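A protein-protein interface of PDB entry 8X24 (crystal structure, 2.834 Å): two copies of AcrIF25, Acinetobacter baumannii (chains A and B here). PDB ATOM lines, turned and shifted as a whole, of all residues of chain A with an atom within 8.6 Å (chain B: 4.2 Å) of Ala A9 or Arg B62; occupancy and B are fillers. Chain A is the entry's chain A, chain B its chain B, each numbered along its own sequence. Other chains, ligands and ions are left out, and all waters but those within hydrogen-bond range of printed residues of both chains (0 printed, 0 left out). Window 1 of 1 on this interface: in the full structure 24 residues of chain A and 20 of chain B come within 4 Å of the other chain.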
ATOM      1  N   ILE A   3     -38.787  21.624  11.804  1.00  0.00           N
ATOM      2  CA  ILE A   3     -38.119  20.934  10.714  1.00  0.00           C
ATOM      3  C   ILE A   3     -36.866  21.671  10.235  1.00  0.00           C
ATOM      4  O   ILE A   3     -36.017  21.076   9.559  1.00  0.00           O
ATOM      5  CB  ILE A   3     -39.112  20.701   9.564  1.00  0.00           C
ATOM      6  CG1 ILE A   3     -38.638  19.528   8.688  1.00  0.00           C
ATOM      7  CG2 ILE A   3     -39.340  21.983   8.779  1.00  0.00           C
ATOM      8  CD1 ILE A   3     -39.639  19.070   7.652  1.00  0.00           C
ATOM      9  N   HIS A   4     -36.707  22.939  10.613  1.00  0.00           N
ATOM     10  CA  HIS A   4     -35.696  23.812  10.010  1.00  0.00           C
ATOM     11  C   HIS A   4     -34.285  23.243  10.125  1.00  0.00           C
ATOM     12  O   HIS A   4     -33.492  23.342   9.183  1.00  0.00           O
ATOM     13  CB  HIS A   4     -35.762  25.186  10.660  1.00  0.00           C
ATOM     14  CG  HIS A   4     -34.718  26.137  10.178  1.00  0.00           C
ATOM     15  ND1 HIS A   4     -34.568  26.461   8.847  1.00  0.00           N
ATOM     16  CD2 HIS A   4     -33.790  26.857  10.853  1.00  0.00           C
ATOM     17  CE1 HIS A   4     -33.590  27.343   8.724  1.00  0.00           C
ATOM     18  NE2 HIS A   4     -33.101  27.599   9.923  1.00  0.00           N
ATOM     19  N   GLU A   5     -33.911  22.729  11.296  1.00  0.00           N
ATOM     20  CA  GLU A   5     -32.555  22.217  11.403  1.00  0.00           C
ATOM     21  C   GLU A   5     -32.388  20.964  10.560  1.00  0.00           C
ATOM     22  O   GLU A   5     -31.321  20.744   9.981  1.00  0.00           O
ATOM     23  CB  GLU A   5     -32.206  21.933  12.860  1.00  0.00           C
ATOM     24  CG  GLU A   5     -31.793  23.155  13.672  1.00  0.00           C
ATOM     25  CD  GLU A   5     -30.867  24.109  12.906  1.00  0.00           C
ATOM     26  OE1 GLU A   5     -29.786  23.669  12.430  1.00  0.00           O
ATOM     27  OE2 GLU A   5     -31.209  25.312  12.806  1.00  0.00           O
ATOM     28  N   PHE A   6     -33.454  20.175  10.423  1.00  0.00           N
ATOM     29  CA  PHE A   6     -33.404  18.977   9.591  1.00  0.00           C
ATOM     30  C   PHE A   6     -33.227  19.339   8.133  1.00  0.00           C
ATOM     31  O   PHE A   6     -32.524  18.639   7.401  1.00  0.00           O
ATOM     32  CB  PHE A   6     -34.676  18.151   9.766  1.00  0.00           C
ATOM     33  CG  PHE A   6     -34.785  17.472  11.092  1.00  0.00           C
ATOM     34  CD1 PHE A   6     -34.011  16.359  11.382  1.00  0.00           C
ATOM     35  CD2 PHE A   6     -35.660  17.949  12.050  1.00  0.00           C
ATOM     36  CE1 PHE A   6     -34.119  15.727  12.602  1.00  0.00           C
ATOM     37  CE2 PHE A   6     -35.773  17.324  13.264  1.00  0.00           C
ATOM     38  CZ  PHE A   6     -35.001  16.211  13.543  1.00  0.00           C
ATOM     39  N   GLY A   7     -33.918  20.390   7.685  1.00  0.00           N
ATOM     40  CA  GLY A   7     -33.761  20.841   6.317  1.00  0.00           C
ATOM     41  C   GLY A   7     -32.345  21.304   6.050  1.00  0.00           C
ATOM     42  O   GLY A   7     -31.799  21.069   4.974  1.00  0.00           O
ATOM     43  N   LEU A   8     -31.732  21.982   7.023  1.00  0.00           N
ATOM     44  CA  LEU A   8     -30.347  22.398   6.854  1.00  0.00           C
ATOM     45  C   LEU A   8     -29.431  21.193   6.738  1.00  0.00           C
ATOM     46  O   LEU A   8     -28.572  21.130   5.849  1.00  0.00           O
ATOM     47  CB  LEU A   8     -29.909  23.258   8.036  1.00  0.00           C
ATOM     48  CG  LEU A   8     -30.513  24.650   8.212  1.00  0.00           C
ATOM     49  CD1 LEU A   8     -29.636  25.486   9.118  1.00  0.00           C
ATOM     50  CD2 LEU A   8     -30.707  25.325   6.867  1.00  0.00           C
ATOM     51  N   ALA A   9     -29.658  20.186   7.571  1.00  0.00           N
ATOM     52  CA  ALA A   9     -28.742  19.054   7.592  1.00  0.00           C
ATOM     53  C   ALA A   9     -28.950  18.163   6.389  1.00  0.00           C
ATOM     54  O   ALA A   9     -27.993  17.565   5.892  1.00  0.00           O
ATOM     55  CB  ALA A   9     -28.896  18.246   8.884  1.00  0.00           C
ATOM     56  N   LEU A  10     -30.192  18.039   5.934  1.00  0.00           N
ATOM     57  CA  LEU A  10     -30.519  17.161   4.820  1.00  0.00           C
ATOM     58  C   LEU A  10     -30.425  17.836   3.464  1.00  0.00           C
ATOM     59  O   LEU A  10     -30.228  17.129   2.470  1.00  0.00           O
ATOM     60  CB  LEU A  10     -31.919  16.588   5.005  1.00  0.00           C
ATOM     61  CG  LEU A  10     -31.946  15.687   6.236  1.00  0.00           C
ATOM     62  CD1 LEU A  10     -33.311  15.090   6.477  1.00  0.00           C
ATOM     63  CD2 LEU A  10     -30.889  14.581   6.087  1.00  0.00           C
ATOM     64  N   PHE A  11     -30.736  19.118   3.360  1.00  0.00           N
ATOM     65  CA  PHE A  11     -30.806  19.700   1.999  1.00  0.00           C
ATOM     66  C   PHE A  11     -30.131  21.063   1.916  1.00  0.00           C
ATOM     67  O   PHE A  11     -30.064  21.606   0.846  1.00  0.00           O
ATOM     68  CB  PHE A  11     -32.259  19.749   1.532  1.00  0.00           C
ATOM     69  CG  PHE A  11     -32.996  18.439   1.641  1.00  0.00           C
ATOM     70  CD1 PHE A  11     -32.671  17.374   0.827  1.00  0.00           C
ATOM     71  CD2 PHE A  11     -34.014  18.269   2.555  1.00  0.00           C
ATOM     72  CE1 PHE A  11     -33.346  16.176   0.934  1.00  0.00           C
ATOM     73  CE2 PHE A  11     -34.686  17.068   2.653  1.00  0.00           C
ATOM     74  CZ  PHE A  11     -34.347  16.027   1.845  1.00  0.00           C
ATOM     75  N   GLY A  12     -29.719  21.616   3.043  1.00  0.00           N
ATOM     76  CA  GLY A  12     -28.993  22.890   3.006  1.00  0.00           C
ATOM     77  C   GLY A  12     -29.844  24.108   3.245  1.00  0.00           C
ATOM     78  O   GLY A  12     -30.912  23.995   3.748  1.00  0.00           O
ATOM     79  N   GLU A  13     -29.331  25.252   2.853  1.00  0.00           N
ATOM     80  CA  GLU A  13     -30.009  26.538   3.073  1.00  0.00           C
ATOM     81  C   GLU A  13     -31.292  26.610   2.256  1.00  0.00           C
ATOM     82  O   GLU A  13     -32.257  27.145   2.755  1.00  0.00           O
ATOM     83  CB  GLU A  13     -29.075  27.647   2.600  1.00  0.00           C
ATOM     84  CG  GLU A  13     -28.714  28.664   3.661  1.00  0.00           C
ATOM     85  CD  GLU A  13     -28.578  30.088   3.152  1.00  0.00           C
ATOM     86  OE1 GLU A  13     -29.606  30.702   2.830  1.00  0.00           O
ATOM     87  OE2 GLU A  13     -27.447  30.585   3.092  1.00  0.00           O
ATOM     88  N   HIS A  14     -31.298  26.051   1.056  1.00  0.00           N
ATOM     89  CA  HIS A  14     -32.469  26.248   0.174  1.00  0.00           C
ATOM     90  C   HIS A  14     -33.341  25.016   0.071  1.00  0.00           C
ATOM     91  O   HIS A  14     -33.814  24.748  -1.024  1.00  0.00           O
ATOM     92  CB  HIS A  14     -31.987  26.642  -1.200  1.00  0.00           C
ATOM     93  CG  HIS A  14     -31.387  27.994  -1.199  1.00  0.00           C
ATOM     94  ND1 HIS A  14     -30.046  28.189  -1.130  1.00  0.00           N
ATOM     95  CD2 HIS A  14     -31.954  29.206  -1.234  1.00  0.00           C
ATOM     96  CE1 HIS A  14     -29.798  29.465  -1.136  1.00  0.00           C
ATOM     97  NE2 HIS A  14     -30.947  30.103  -1.199  1.00  0.00           N
ATOM     98  N   TYR A  15     -33.598  24.379   1.203  1.00  0.00           N
ATOM     99  CA  TYR A  15     -34.416  23.153   1.261  1.00  0.00           C
ATOM    100  C   TYR A  15     -35.864  23.494   0.956  1.00  0.00           C
ATOM    101  O   TYR A  15     -36.294  24.562   1.255  1.00  0.00           O
ATOM    102  CB  TYR A  15     -34.249  22.494   2.623  1.00  0.00           C
ATOM    103  CG  TYR A  15     -34.813  23.268   3.777  1.00  0.00           C
ATOM    104  CD1 TYR A  15     -36.133  23.139   4.134  1.00  0.00           C
ATOM    105  CD2 TYR A  15     -34.028  24.127   4.509  1.00  0.00           C
ATOM    106  CE1 TYR A  15     -36.662  23.845   5.191  1.00  0.00           C
ATOM    107  CE2 TYR A  15     -34.534  24.834   5.574  1.00  0.00           C
ATOM    108  CZ  TYR A  15     -35.858  24.696   5.912  1.00  0.00           C
ATOM    109  OH  TYR A  15     -36.369  25.388   6.956  1.00  0.00           O
ATOM    110  N   GLN A  19     -38.556  18.101  -1.257  1.00  0.00           N
ATOM    111  CA  GLN A  19     -37.447  17.205  -0.958  1.00  0.00           C
ATOM    112  C   GLN A  19     -37.797  16.282   0.203  1.00  0.00           C
ATOM    113  O   GLN A  19     -37.317  15.138   0.268  1.00  0.00           O
ATOM    114  CB  GLN A  19     -36.209  18.035  -0.635  1.00  0.00           C
ATOM    115  CG  GLN A  19     -36.217  19.369  -1.344  1.00  0.00           C
ATOM    116  CD  GLN A  19     -34.863  20.004  -1.424  1.00  0.00           C
ATOM    117  OE1 GLN A  19     -33.838  19.350  -1.206  1.00  0.00           O
ATOM    118  NE2 GLN A  19     -34.840  21.291  -1.770  1.00  0.00           N
ATOM    119  N   PHE A  20     -38.620  16.773   1.134  1.00  0.00           N
ATOM    120  CA  PHE A  20     -39.075  15.959   2.246  1.00  0.00           C
ATOM    121  C   PHE A  20     -40.136  14.969   1.807  1.00  0.00           C
ATOM    122  O   PHE A  20     -40.149  13.837   2.298  1.00  0.00           O
ATOM    123  CB  PHE A  20     -39.605  16.845   3.372  1.00  0.00           C
ATOM    124  CG  PHE A  20     -38.530  17.368   4.289  1.00  0.00           C
ATOM    125  CD1 PHE A  20     -37.832  16.507   5.135  1.00  0.00           C
ATOM    126  CD2 PHE A  20     -38.203  18.720   4.302  1.00  0.00           C
ATOM    127  CE1 PHE A  20     -36.838  16.988   5.988  1.00  0.00           C
ATOM    128  CE2 PHE A  20     -37.208  19.207   5.150  1.00  0.00           C
ATOM    129  CZ  PHE A  20     -36.528  18.342   5.997  1.00  0.00           C
ATOM    130  N   LEU A  55     -36.975  11.310  10.240  1.00  0.00           N
ATOM    131  CA  LEU A  55     -35.889  12.221   9.925  1.00  0.00           C
ATOM    132  C   LEU A  55     -34.609  11.798  10.625  1.00  0.00           C
ATOM    133  O   LEU A  55     -33.520  11.898  10.051  1.00  0.00           O
ATOM    134  CB  LEU A  55     -36.281  13.648  10.288  1.00  0.00           C
ATOM    135  CG  LEU A  55     -37.478  14.181   9.490  1.00  0.00           C
ATOM    136  CD1 LEU A  55     -37.699  15.666   9.727  1.00  0.00           C
ATOM    137  CD2 LEU A  55     -37.304  13.920   8.018  1.00  0.00           C
ATOM    138  N   GLU A  58     -32.927   9.423   8.524  1.00  0.00           N
ATOM    139  CA  GLU A  58     -32.248  10.054   7.404  1.00  0.00           C
ATOM    140  C   GLU A  58     -30.903  10.630   7.798  1.00  0.00           C
ATOM    141  O   GLU A  58     -29.915  10.454   7.079  1.00  0.00           O
ATOM    142  CB  GLU A  58     -33.142  11.120   6.777  1.00  0.00           C
ATOM    143  CG  GLU A  58     -34.251  10.463   6.017  1.00  0.00           C
ATOM    144  CD  GLU A  58     -33.713   9.470   4.955  1.00  0.00           C
ATOM    145  OE1 GLU A  58     -32.546   9.614   4.462  1.00  0.00           O
ATOM    146  OE2 GLU A  58     -34.459   8.504   4.654  1.00  0.00           O
ATOM    147  N   LEU A  59     -30.842  11.318   8.935  1.00  0.00           N
ATOM    148  CA  LEU A  59     -29.573  11.868   9.385  1.00  0.00           C
ATOM    149  C   LEU A  59     -28.530  10.769   9.529  1.00  0.00           C
ATOM    150  O   LEU A  59     -27.409  10.879   9.017  1.00  0.00           O
ATOM    151  CB  LEU A  59     -29.782  12.574  10.714  1.00  0.00           C
ATOM    152  CG  LEU A  59     -30.752  13.738  10.647  1.00  0.00           C
ATOM    153  CD1 LEU A  59     -30.985  14.342  12.017  1.00  0.00           C
ATOM    154  CD2 LEU A  59     -30.165  14.756   9.719  1.00  0.00           C
ATOM    155  N   ARG A  62     -27.293   9.357   6.209  1.00  0.00           N
ATOM    156  CA  ARG A  62     -26.474  10.315   5.473  1.00  0.00           C
ATOM    157  C   ARG A  62     -25.069  10.407   6.031  1.00  0.00           C
ATOM    158  O   ARG A  62     -24.102  10.443   5.262  1.00  0.00           O
ATOM    159  CB  ARG A  62     -27.102  11.690   5.530  1.00  0.00           C
ATOM    160  CG  ARG A  62     -28.185  11.923   4.570  1.00  0.00           C
ATOM    161  CD  ARG A  62     -27.670  12.208   3.181  1.00  0.00           C
ATOM    162  NE  ARG A  62     -28.593  13.100   2.481  1.00  0.00           N
ATOM    163  CZ  ARG A  62     -29.918  12.968   2.399  1.00  0.00           C
ATOM    164  NH1 ARG A  62     -30.558  11.889   2.873  1.00  0.00           N
ATOM    165  NH2 ARG A  62     -30.627  13.956   1.855  1.00  0.00           N
ATOM    166  N   GLU A  63     -24.922  10.428   7.360  1.00  0.00           N
ATOM    167  CA  GLU A  63     -23.576  10.475   7.915  1.00  0.00           C
ATOM    168  C   GLU A  63     -22.736   9.365   7.329  1.00  0.00           C
ATOM    169  O   GLU A  63     -21.589   9.585   6.924  1.00  0.00           O
ATOM    170  CB  GLU A  63     -23.602  10.375   9.430  1.00  0.00           C
ATOM    171  CG  GLU A  63     -22.722  11.401  10.097  1.00  0.00           C
ATOM    172  CD  GLU A  63     -22.544  11.152  11.589  1.00  0.00           C
ATOM    173  OE1 GLU A  63     -23.158  10.191  12.120  1.00  0.00           O
ATOM    174  OE2 GLU A  63     -21.794  11.924  12.237  1.00  0.00           O
ATOM    175  N   LEU A  66     -22.066  10.295   3.704  1.00  0.00           N
ATOM    176  CA  LEU A  66     -21.235  11.516   3.670  1.00  0.00           C
ATOM    177  C   LEU A  66     -19.850  11.287   4.248  1.00  0.00           C
ATOM    178  O   LEU A  66     -18.932  11.786   3.669  1.00  0.00           O
ATOM    179  CB  LEU A  66     -21.944  12.663   4.387  1.00  0.00           C
ATOM    180  CG  LEU A  66     -21.167  13.971   4.374  1.00  0.00           C
ATOM    181  CD1 LEU A  66     -22.015  15.113   3.917  1.00  0.00           C
ATOM    182  CD2 LEU A  66     -20.576  14.269   5.719  1.00  0.00           C
ATOM    183  N   LEU A  70     -16.014  11.417   1.956  1.00  0.00           N
ATOM    184  CA  LEU A  70     -14.918  12.283   2.444  1.00  0.00           C
ATOM    185  C   LEU A  70     -13.621  11.492   2.609  1.00  0.00           C
ATOM    186  O   LEU A  70     -12.573  12.090   2.510  1.00  0.00           O
ATOM    187  CB  LEU A  70     -15.345  12.851   3.792  1.00  0.00           C
ATOM    188  CG  LEU A  70     -16.178  14.123   3.769  1.00  0.00           C
ATOM    189  CD1 LEU A  70     -16.393  14.612   5.175  1.00  0.00           C
ATOM    190  CD2 LEU A  70     -15.514  15.194   2.937  1.00  0.00           C
ATOM    191  N   LEU B  10     -25.154  15.283  -0.499  1.00  0.00           N
ATOM    192  CA  LEU B  10     -25.649  16.639  -0.265  1.00  0.00           C
ATOM    193  C   LEU B  10     -27.163  16.762  -0.396  1.00  0.00           C
ATOM    194  O   LEU B  10     -27.744  17.662   0.215  1.00  0.00           O
ATOM    195  CB  LEU B  10     -24.972  17.635  -1.206  1.00  0.00           C
ATOM    196  CG  LEU B  10     -23.483  17.865  -0.943  1.00  0.00           C
ATOM    197  CD1 LEU B  10     -22.960  18.865  -1.940  1.00  0.00           C
ATOM    198  CD2 LEU B  10     -23.217  18.353   0.478  1.00  0.00           C
ATOM    199  N   PHE B  11     -27.825  15.885  -1.167  1.00  0.00           N
ATOM    200  CA  PHE B  11     -29.250  16.053  -1.440  1.00  0.00           C
ATOM    201  C   PHE B  11     -30.082  14.765  -1.452  1.00  0.00           C
ATOM    202  O   PHE B  11     -31.304  14.857  -1.624  1.00  0.00           O
ATOM    203  CB  PHE B  11     -29.450  16.769  -2.785  1.00  0.00           C
ATOM    204  CG  PHE B  11     -28.663  18.039  -2.928  1.00  0.00           C
ATOM    205  CD1 PHE B  11     -28.898  19.115  -2.092  1.00  0.00           C
ATOM    206  CD2 PHE B  11     -27.696  18.161  -3.905  1.00  0.00           C
ATOM    207  CE1 PHE B  11     -28.179  20.274  -2.218  1.00  0.00           C
ATOM    208  CE2 PHE B  11     -26.975  19.327  -4.032  1.00  0.00           C
ATOM    209  CZ  PHE B  11     -27.219  20.381  -3.183  1.00  0.00           C
ATOM    210  N   GLU B  58     -18.409  21.971   0.709  1.00  0.00           N
ATOM    211  CA  GLU B  58     -19.784  21.788   1.140  1.00  0.00           C
ATOM    212  C   GLU B  58     -19.916  20.541   1.995  1.00  0.00           C
ATOM    213  O   GLU B  58     -20.575  20.573   3.038  1.00  0.00           O
ATOM    214  CB  GLU B  58     -20.710  21.737  -0.069  1.00  0.00           C
ATOM    215  CG  GLU B  58     -21.479  23.045  -0.330  1.00  0.00           C
ATOM    216  CD  GLU B  58     -22.329  23.517   0.869  1.00  0.00           C
ATOM    217  OE1 GLU B  58     -23.149  22.695   1.387  1.00  0.00           O
ATOM    218  OE2 GLU B  58     -22.205  24.722   1.253  1.00  0.00           O
ATOM    219  N   LEU B  59     -19.258  19.462   1.607  1.00  0.00           N
ATOM    220  CA  LEU B  59     -19.348  18.197   2.374  1.00  0.00           C
ATOM    221  C   LEU B  59     -18.765  18.376   3.771  1.00  0.00           C
ATOM    222  O   LEU B  59     -19.311  17.865   4.708  1.00  0.00           O
ATOM    223  CB  LEU B  59     -18.571  17.105   1.647  1.00  0.00           C
ATOM    224  CG  LEU B  59     -19.087  16.674   0.288  1.00  0.00           C
ATOM    225  CD1 LEU B  59     -18.160  15.626  -0.285  1.00  0.00           C
ATOM    226  CD2 LEU B  59     -20.497  16.138   0.389  1.00  0.00           C
ATOM    227  N   LEU B  60     -17.664  19.086   3.896  1.00  0.00           N
ATOM    228  CA  LEU B  60     -17.070  19.266   5.233  1.00  0.00           C
ATOM    229  C   LEU B  60     -17.919  20.213   6.071  1.00  0.00           C
ATOM    230  O   LEU B  60     -17.854  20.129   7.273  1.00  0.00           O
ATOM    231  CB  LEU B  60     -15.669  19.828   5.060  1.00  0.00           C
ATOM    232  CG  LEU B  60     -14.658  18.840   4.522  1.00  0.00           C
ATOM    233  CD1 LEU B  60     -13.350  19.539   4.277  1.00  0.00           C
ATOM    234  CD2 LEU B  60     -14.479  17.703   5.483  1.00  0.00           C
ATOM    235  N   LYS B  61     -18.616  21.140   5.441  1.00  0.00           N
ATOM    236  CA  LYS B  61     -19.489  22.073   6.182  1.00  0.00           C
ATOM    237  C   LYS B  61     -20.720  21.311   6.668  1.00  0.00           C
ATOM    238  O   LYS B  61     -21.093  21.497   7.798  1.00  0.00           O
ATOM    239  CB  LYS B  61     -19.885  23.222   5.260  1.00  0.00           C
ATOM    240  CG  LYS B  61     -18.932  24.396   5.187  1.00  0.00           C
ATOM    241  CD  LYS B  61     -19.484  25.455   4.293  1.00  0.00           C
ATOM    242  CE  LYS B  61     -18.469  26.050   3.349  1.00  0.00           C
ATOM    243  NZ  LYS B  61     -18.917  26.013   1.940  1.00  0.00           N
ATOM    244  N   ARG B  62     -21.293  20.461   5.822  1.00  0.00           N
ATOM    245  CA  ARG B  62     -22.514  19.681   6.146  1.00  0.00           C
ATOM    246  C   ARG B  62     -22.235  18.642   7.224  1.00  0.00           C
ATOM    247  O   ARG B  62     -23.092  18.445   8.033  1.00  0.00           O
ATOM    248  CB  ARG B  62     -23.101  19.035   4.897  1.00  0.00           C
ATOM    249  CG  ARG B  62     -24.603  18.858   4.972  1.00  0.00           C
ATOM    250  CD  ARG B  62     -25.276  20.175   4.755  1.00  0.00           C
ATOM    251  NE  ARG B  62     -25.607  20.324   3.360  1.00  0.00           N
ATOM    252  CZ  ARG B  62     -26.431  19.553   2.702  1.00  0.00           C
ATOM    253  NH1 ARG B  62     -26.866  18.451   3.252  1.00  0.00           N
ATOM    254  NH2 ARG B  62     -26.791  19.854   1.481  1.00  0.00           N
ATOM    255  N   GLU B  63     -21.055  18.038   7.231  1.00  0.00           N
ATOM    256  CA  GLU B  63     -20.651  17.056   8.263  1.00  0.00           C
ATOM    257  C   GLU B  63     -20.689  17.695   9.652  1.00  0.00           C
ATOM    258  O   GLU B  63     -21.073  17.033  10.577  1.00  0.00           O
ATOM    259  CB  GLU B  63     -19.237  16.595   7.951  1.00  0.00           C
ATOM    260  CG  GLU B  63     -18.831  15.332   8.668  1.00  0.00           C
ATOM    261  CD  GLU B  63     -17.340  15.233   8.922  1.00  0.00           C
ATOM    262  OE1 GLU B  63     -16.632  16.202   8.630  1.00  0.00           O
ATOM    263  OE2 GLU B  63     -16.895  14.184   9.391  1.00  0.00           O
ATOM    264  N   VAL B  64     -20.275  18.949   9.771  1.00  0.00           N
ATOM    265  CA  VAL B  64     -20.274  19.693  11.059  1.00  0.00           C
ATOM    266  C   VAL B  64     -21.708  19.912  11.529  1.00  0.00           C
ATOM    267  O   VAL B  64     -21.978  19.638  12.673  1.00  0.00           O
ATOM    268  CB  VAL B  64     -19.529  21.034  10.928  1.00  0.00           C
ATOM    269  CG1 VAL B  64     -19.853  21.958  12.077  1.00  0.00           C
ATOM    270  CG2 VAL B  64     -18.036  20.841  10.852  1.00  0.00           C
ATOM    271  N   ILE B  65     -22.571  20.397  10.648  1.00  0.00           N
ATOM    272  CA  ILE B  65     -23.995  20.698  10.945  1.00  0.00           C
ATOM    273  C   ILE B  65     -24.725  19.413  11.330  1.00  0.00           C
ATOM    274  O   ILE B  65     -25.466  19.420  12.295  1.00  0.00           O
ATOM    275  CB  ILE B  65     -24.603  21.348   9.696  1.00  0.00           C
ATOM    276  CG1 ILE B  65     -23.974  22.708   9.420  1.00  0.00           C
ATOM    277  CG2 ILE B  65     -26.112  21.432   9.777  1.00  0.00           C
ATOM    278  CD1 ILE B  65     -24.487  23.357   8.179  1.00  0.00           C
ATOM    279  N   LEU B  66     -24.513  18.355  10.566  1.00  0.00           N
ATOM    280  CA  LEU B  66     -25.151  17.041  10.779  1.00  0.00           C
ATOM    281  C   LEU B  66     -24.683  16.453  12.098  1.00  0.00           C
ATOM    282  O   LEU B  66     -25.455  15.797  12.717  1.00  0.00           O
ATOM    283  CB  LEU B  66     -24.682  16.164   9.625  1.00  0.00           C
ATOM    284  CG  LEU B  66     -25.561  15.016   9.168  1.00  0.00           C
ATOM    285  CD1 LEU B  66     -26.879  15.524   8.660  1.00  0.00           C
ATOM    286  CD2 LEU B  66     -24.851  14.304   8.054  1.00  0.00           C
ATOM    287  N   LEU B  69     -26.466  18.294  15.029  1.00  0.00           N
ATOM    288  CA  LEU B  69     -27.834  17.812  15.130  1.00  0.00           C
ATOM    289  C   LEU B  69     -27.894  16.436  15.763  1.00  0.00           C
ATOM    290  O   LEU B  69     -28.696  16.200  16.671  1.00  0.00           O
ATOM    291  CB  LEU B  69     -28.485  17.767  13.758  1.00  0.00           C
ATOM    292  CG  LEU B  69     -29.963  18.050  13.914  1.00  0.00           C
ATOM    293  CD1 LEU B  69     -30.073  19.487  14.379  1.00  0.00           C
ATOM    294  CD2 LEU B  69     -30.690  17.830  12.599  1.00  0.00           C
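Leu A8 touches Arg B62 (O to CD, 3.6 Å). O of Phe B11 touches CE1 of Phe A11, 3.5 Å away. Arg B62 touches Phe A11 (NH2 to C, 3.6 Å). CD1 of Leu B66 touches CD2 of Leu A59 (3.5 Å). Leu B69 touches Leu A59. C of Phe B11 touches NH2 of Arg A62 (3.4 Å). N of Glu A63 touches CD2 of Leu B66, at 3.9 Å. Glu B63 touches Leu A66 (CB to CD2, 3.5 Å). Leu A70 touches Leu B59 (CD2 to CB, 3.8 Å). Leu A70 touches Glu B63 (CD1 to OE1, 3.8 Å).
Of the 12 printed residues of chain B, 8 touch a printed residue of chain A. Printed residues of chain A that touch a printed residue of chain B: Glu A5, Phe A6, Leu A8, Ala A9, Leu A10, Phe A11, Gly A12, Leu A59, Arg A62, Glu A63, Leu A66 and Leu A70. Hydrophobic or aromatic side chains of chain A within 4 Å of the printed part of chain B: Phe A6, Ala A9, Phe A11, Leu A59, Leu A66 and Leu A70.
The backbone carbonyl oxygen (O) of Ala A9 is in hydrogen-bond range of the guanidinium group (NH1) of Arg B62 (3.0 Å). The backbone carbonyl oxygen (O) of Leu A10 lies close to the backbone carbonyl oxygen (O) of Leu B10 (3.4 Å).
The backbone NH (N) of Gly A12 lies within hydrogen-bond range of the backbone carbonyl oxygen (O) of Gly A7, 2.9 Å away. NH2 of Arg B62 is in hydrogen-bond range of O of Leu B10. NE of Arg B62 lies within salt-bridge range of OE1 of Glu B58 (3.9 Å). The backbone carbonyl oxygen of Leu A10 sits at hydrogen-bond distance from the guanidinium group of Arg A62 (3.3 Å). The guanidinium group (NH1) of Arg A62 is in salt-bridge range of the side-chain carboxylate (OE1) of Glu A58, at 3.4 Å.
Leu B10 touches its own counterpart, Leu A10. Phe A11 touches its own counterpart, Phe B11. Leu A59 touches Leu B66, and with the chains exchanged Leu A66 touches Leu B59. Glu A63 touches Leu B66, and with the chains exchanged Leu A66 touches Glu B63. Positions printed for both chains: 10, 11, 58, 59, 62, 63 and 66. Of the 19 pairs that touch across the chains among the printed residues, 8 have their exchanged pair printed and touching as well.
Ala A9 touches just these residues of chain B: Arg B62 and Leu B66. Tyr A15 touches none of the printed residues of chain B. Leu A55 touches none of the printed residues of chain B. Of the printed residues of chain B, Leu A59 touches Leu B66 and Leu B69. Printed residues of chain B within 4 Å of Arg A62: Phe B11 (3.4 Å). Of the printed residues of chain B, Glu A63 touches Leu B66. Of the printed residues of chain A, Leu B10 touches Leu A10 (3.4 Å). Of the printed residues of chain A, Leu B60 touches Leu A70. Arg B62 touches just these residues of chain A: Leu A8, Ala A9, Leu A10, Phe A11 and Gly A12. The nearest printed residue of chain B that does not touch Ala A9 is Leu B69 (4.1 Å). The nearest printed residue of chain B that does not touch Leu A70 is Lys B61 (6.9 Å).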
